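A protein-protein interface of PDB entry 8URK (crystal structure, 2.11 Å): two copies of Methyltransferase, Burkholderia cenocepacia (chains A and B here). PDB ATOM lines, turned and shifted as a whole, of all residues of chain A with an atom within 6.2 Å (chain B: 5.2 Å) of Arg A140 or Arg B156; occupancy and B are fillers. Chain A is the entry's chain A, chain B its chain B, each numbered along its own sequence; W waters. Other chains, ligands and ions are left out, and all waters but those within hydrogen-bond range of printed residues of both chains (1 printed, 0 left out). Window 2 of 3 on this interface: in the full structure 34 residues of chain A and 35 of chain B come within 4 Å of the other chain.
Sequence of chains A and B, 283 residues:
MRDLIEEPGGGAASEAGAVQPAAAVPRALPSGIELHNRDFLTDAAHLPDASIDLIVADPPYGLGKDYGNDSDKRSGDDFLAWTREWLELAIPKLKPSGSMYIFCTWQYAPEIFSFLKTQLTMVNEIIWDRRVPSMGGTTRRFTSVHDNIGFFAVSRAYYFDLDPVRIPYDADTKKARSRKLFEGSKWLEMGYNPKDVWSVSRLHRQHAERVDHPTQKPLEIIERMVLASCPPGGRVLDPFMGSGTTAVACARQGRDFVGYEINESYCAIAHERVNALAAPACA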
ATOM      1  N   THR A 138     -31.826   5.249   0.377  1.00  0.00           N
ATOM      2  CA  THR A 138     -30.893   4.143   0.252  1.00  0.00           C
ATOM      3  C   THR A 138     -31.536   2.859  -0.201  1.00  0.00           C
ATOM      4  O   THR A 138     -32.732   2.713  -0.142  1.00  0.00           O
ATOM      5  CB  THR A 138     -30.096   3.904   1.542  1.00  0.00           C
ATOM      6  OG1 THR A 138     -28.946   3.105   1.263  1.00  0.00           O
ATOM      7  CG2 THR A 138     -30.958   3.201   2.570  1.00  0.00           C
ATOM      8  N   THR A 139     -30.698   1.946  -0.658  1.00  0.00           N
ATOM      9  CA  THR A 139     -31.146   0.662  -1.163  1.00  0.00           C
ATOM     10  C   THR A 139     -30.014  -0.312  -0.844  1.00  0.00           C
ATOM     11  O   THR A 139     -30.118  -1.490  -1.097  1.00  0.00           O
ATOM     12  CB  THR A 139     -31.512   0.799  -2.650  1.00  0.00           C
ATOM     13  OG1 THR A 139     -32.911   1.066  -2.774  1.00  0.00           O
ATOM     14  CG2 THR A 139     -31.166  -0.457  -3.427  1.00  0.00           C
ATOM     15  N   ARG A 140     -28.962   0.184  -0.221  1.00  0.00           N
ATOM     16  CA  ARG A 140     -27.805  -0.621   0.100  1.00  0.00           C
ATOM     17  C   ARG A 140     -27.657  -0.965   1.574  1.00  0.00           C
ATOM     18  O   ARG A 140     -26.579  -1.276   2.016  1.00  0.00           O
ATOM     19  CB  ARG A 140     -26.564   0.096  -0.431  1.00  0.00           C
ATOM     20  CG  ARG A 140     -26.222  -0.243  -1.872  1.00  0.00           C
ATOM     21  CD  ARG A 140     -24.965   0.453  -2.357  1.00  0.00           C
ATOM     22  NE  ARG A 140     -23.753  -0.095  -1.767  1.00  0.00           N
ATOM     23  CZ  ARG A 140     -23.469  -1.389  -1.691  1.00  0.00           C
ATOM     24  NH1 ARG A 140     -24.303  -2.285  -2.175  1.00  0.00           N
ATOM     25  NH2 ARG A 140     -22.346  -1.778  -1.126  1.00  0.00           N
ATOM     26  N   ARG A 141     -28.754  -0.916   2.318  1.00  0.00           N
ATOM     27  CA  ARG A 141     -28.767  -1.266   3.731  1.00  0.00           C
ATOM     28  C   ARG A 141     -30.195  -1.188   4.247  1.00  0.00           C
ATOM     29  O   ARG A 141     -31.078  -0.687   3.590  1.00  0.00           O
ATOM     30  CB  ARG A 141     -27.854  -0.383   4.566  1.00  0.00           C
ATOM     31  CG  ARG A 141     -28.563   0.771   5.251  1.00  0.00           C
ATOM     32  CD  ARG A 141     -27.683   2.003   5.348  1.00  0.00           C
ATOM     33  NE  ARG A 141     -26.588   1.837   6.286  1.00  0.00           N
ATOM     34  CZ  ARG A 141     -25.336   2.192   6.035  1.00  0.00           C
ATOM     35  NH1 ARG A 141     -25.020   2.746   4.874  1.00  0.00           N
ATOM     36  NH2 ARG A 141     -24.398   2.002   6.940  1.00  0.00           N
ATOM     37  N   PHE A 142     -30.408  -1.694   5.439  1.00  0.00           N
ATOM     38  CA  PHE A 142     -31.724  -1.621   5.992  1.00  0.00           C
ATOM     39  C   PHE A 142     -32.014  -0.229   6.563  1.00  0.00           C
ATOM     40  O   PHE A 142     -31.179   0.387   7.158  1.00  0.00           O
ATOM     41  CB  PHE A 142     -31.968  -2.762   6.982  1.00  0.00           C
ATOM     42  CG  PHE A 142     -31.768  -4.114   6.396  1.00  0.00           C
ATOM     43  CD1 PHE A 142     -32.777  -4.726   5.684  1.00  0.00           C
ATOM     44  CD2 PHE A 142     -30.568  -4.769   6.546  1.00  0.00           C
ATOM     45  CE1 PHE A 142     -32.593  -5.975   5.135  1.00  0.00           C
ATOM     46  CE2 PHE A 142     -30.376  -6.016   5.998  1.00  0.00           C
ATOM     47  CZ  PHE A 142     -31.390  -6.620   5.291  1.00  0.00           C
ATOM     48  N   VAL B 123     -22.646  -1.746   8.812  1.00  0.00           N
ATOM     49  CA  VAL B 123     -23.614  -1.181   7.913  1.00  0.00           C
ATOM     50  C   VAL B 123     -24.939  -0.986   8.637  1.00  0.00           C
ATOM     51  O   VAL B 123     -25.584   0.041   8.490  1.00  0.00           O
ATOM     52  CB  VAL B 123     -23.789  -2.075   6.673  1.00  0.00           C
ATOM     53  CG1 VAL B 123     -24.986  -1.651   5.842  1.00  0.00           C
ATOM     54  CG2 VAL B 123     -22.512  -2.134   5.851  1.00  0.00           C
ATOM     55  N   VAL B 154     -16.745  -6.149   4.884  1.00  0.00           N
ATOM     56  CA  VAL B 154     -15.301  -5.978   4.743  1.00  0.00           C
ATOM     57  C   VAL B 154     -14.943  -4.641   4.094  1.00  0.00           C
ATOM     58  O   VAL B 154     -14.093  -3.938   4.587  1.00  0.00           O
ATOM     59  CB  VAL B 154     -14.671  -7.143   3.959  1.00  0.00           C
ATOM     60  CG1 VAL B 154     -13.310  -6.749   3.421  1.00  0.00           C
ATOM     61  CG2 VAL B 154     -14.587  -8.391   4.817  1.00  0.00           C
ATOM     62  N   SER B 155     -15.627  -4.298   3.017  1.00  0.00           N
ATOM     63  CA  SER B 155     -15.318  -3.069   2.300  1.00  0.00           C
ATOM     64  C   SER B 155     -16.534  -2.290   1.894  1.00  0.00           C
ATOM     65  O   SER B 155     -17.645  -2.777   1.942  1.00  0.00           O
ATOM     66  CB  SER B 155     -14.469  -3.359   1.047  1.00  0.00           C
ATOM     67  OG  SER B 155     -13.180  -3.819   1.388  1.00  0.00           O
ATOM     68  N   ARG B 156     -16.302  -1.070   1.457  1.00  0.00           N
ATOM     69  CA  ARG B 156     -17.418  -0.214   1.091  1.00  0.00           C
ATOM     70  C   ARG B 156     -18.192  -0.763  -0.097  1.00  0.00           C
ATOM     71  O   ARG B 156     -19.366  -0.414  -0.277  1.00  0.00           O
ATOM     72  CB  ARG B 156     -16.908   1.194   0.789  1.00  0.00           C
ATOM     73  CG  ARG B 156     -15.713   1.590   1.646  1.00  0.00           C
ATOM     74  CD  ARG B 156     -14.866   2.621   0.936  1.00  0.00           C
ATOM     75  NE  ARG B 156     -15.670   3.769   0.536  1.00  0.00           N
ATOM     76  CZ  ARG B 156     -15.288   5.032   0.662  1.00  0.00           C
ATOM     77  NH1 ARG B 156     -14.114   5.351   1.190  1.00  0.00           N
ATOM     78  NH2 ARG B 156     -16.104   5.999   0.248  1.00  0.00           N
ATOM     79  N   ALA B 157     -17.570  -1.650  -0.846  1.00  0.00           N
ATOM     80  CA  ALA B 157     -18.199  -2.224  -1.997  1.00  0.00           C
ATOM     81  C   ALA B 157     -18.794  -3.595  -1.744  1.00  0.00           C
ATOM     82  O   ALA B 157     -18.620  -4.502  -2.538  1.00  0.00           O
ATOM     83  CB  ALA B 157     -17.158  -2.313  -3.074  1.00  0.00           C
ATOM     84  N   TYR B 158     -19.512  -3.746  -0.659  1.00  0.00           N
ATOM     85  CA  TYR B 158     -20.091  -5.006  -0.324  1.00  0.00           C
ATOM     86  C   TYR B 158     -21.276  -5.304  -1.173  1.00  0.00           C
ATOM     87  O   TYR B 158     -22.022  -4.427  -1.528  1.00  0.00           O
ATOM     88  CB  TYR B 158     -20.498  -5.004   1.175  1.00  0.00           C
ATOM     89  CG  TYR B 158     -21.444  -3.904   1.556  1.00  0.00           C
ATOM     90  CD1 TYR B 158     -20.972  -2.671   1.956  1.00  0.00           C
ATOM     91  CD2 TYR B 158     -22.808  -4.096   1.508  1.00  0.00           C
ATOM     92  CE1 TYR B 158     -21.834  -1.657   2.295  1.00  0.00           C
ATOM     93  CE2 TYR B 158     -23.678  -3.086   1.844  1.00  0.00           C
ATOM     94  CZ  TYR B 158     -23.180  -1.873   2.239  1.00  0.00           C
ATOM     95  OH  TYR B 158     -24.034  -0.869   2.578  1.00  0.00           O
ATOM     96  N   TYR B 159     -21.473  -6.564  -1.470  1.00  0.00           N
ATOM     97  CA  TYR B 159     -22.634  -6.958  -2.208  1.00  0.00           C
ATOM     98  C   TYR B 159     -23.866  -6.841  -1.365  1.00  0.00           C
ATOM     99  O   TYR B 159     -23.846  -7.209  -0.216  1.00  0.00           O
ATOM    100  CB  TYR B 159     -22.513  -8.385  -2.700  1.00  0.00           C
ATOM    101  CG  TYR B 159     -23.780  -8.962  -3.253  1.00  0.00           C
ATOM    102  CD1 TYR B 159     -24.140  -8.746  -4.569  1.00  0.00           C
ATOM    103  CD2 TYR B 159     -24.619  -9.727  -2.463  1.00  0.00           C
ATOM    104  CE1 TYR B 159     -25.301  -9.271  -5.083  1.00  0.00           C
ATOM    105  CE2 TYR B 159     -25.784 -10.252  -2.967  1.00  0.00           C
ATOM    106  CZ  TYR B 159     -26.117 -10.020  -4.280  1.00  0.00           C
ATOM    107  OH  TYR B 159     -27.273 -10.536  -4.792  1.00  0.00           O
ATOM    108  N   PHE B 160     -24.935  -6.355  -1.956  1.00  0.00           N
ATOM    109  CA  PHE B 160     -26.186  -6.174  -1.270  1.00  0.00           C
ATOM    110  C   PHE B 160     -27.296  -5.947  -2.268  1.00  0.00           C
ATOM    111  O   PHE B 160     -27.260  -4.996  -3.019  1.00  0.00           O
ATOM    112  CB  PHE B 160     -26.118  -5.003  -0.277  1.00  0.00           C
ATOM    113  CG  PHE B 160     -27.369  -4.807   0.523  1.00  0.00           C
ATOM    114  CD1 PHE B 160     -28.395  -4.018   0.049  1.00  0.00           C
ATOM    115  CD2 PHE B 160     -27.512  -5.408   1.757  1.00  0.00           C
ATOM    116  CE1 PHE B 160     -29.544  -3.840   0.788  1.00  0.00           C
ATOM    117  CE2 PHE B 160     -28.658  -5.237   2.497  1.00  0.00           C
ATOM    118  CZ  PHE B 160     -29.674  -4.449   2.014  1.00  0.00           C
HETATM  119  O   HOH W   1     -23.481   1.997   2.153  1.00  0.00           O
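The backbone carbonyl oxygen (O) of Arg A140 sits at hydrogen-bond distance from the side-chain hydroxyl (OH) of Tyr B158 (2.6 Å). NH2 of Arg A141 sits at hydrogen-bond distance from O of Val B123 (2.8 Å). O of Arg B156 lies within hydrogen-bond range of NH2 of Arg A140 (3.4 Å).
The side-chain hydroxyl (OG1) of Thr A138 is in hydrogen-bond range of the backbone NH (N) of Arg A140 (3.3 Å).
Among the printed residues, merely in contact across the chains: Thr A139 with Phe B160, Arg A140 with Phe B160, Arg A141 with Phe B160 and Phe A142 with Phe B160.
Thr A138 touches none of the printed residues of chain B. Of the printed residues of chain B, Thr A139 touches Phe B160 (3.1 Å). Arg A140 touches three residues of chain B. Of the printed residues of chain B, Arg A141 touches Val B123 (2.8 Å) and Phe B160 (3.4 Å). Printed residues of chain B within 4 Å of Phe A142: Phe B160. Ser B155 touches none of the printed residues of chain A. Of the printed residues of chain A, Tyr B158 touches Arg A140. Of the printed residues of chain A, Phe B160 touches Thr A139 (3.1 Å), Arg A140 (3.4 Å), Arg A141 (3.4 Å) and Phe A142 (3.98 Å). The nearest residue of chain B that does not touch Arg A140 is Ala B157 (4.04 Å).
Of the 8 printed residues of chain B, 4 touch a printed residue of chain A. Printed residues of chain B that touch a printed residue of chain A: Val B123, Arg B156, Tyr B158 and Phe B160. Hydrophobic or aromatic side chains of chain B within 4 Å of the printed part of chain A: Val B123, Tyr B158 and Phe B160. Hydrophobic or aromatic side chains of chain A that line the printed part of chain B: Phe A142. Among the printed residues, no Asp or Glu carboxylate lies within 4 Å of a Lys or Arg side-chain nitrogen of the other chain.
No position is printed for both chains.
Water W1 lies within hydrogen-bond range of the side-chain hydroxyl of Tyr B158 and the guanidinium group of Arg A141.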
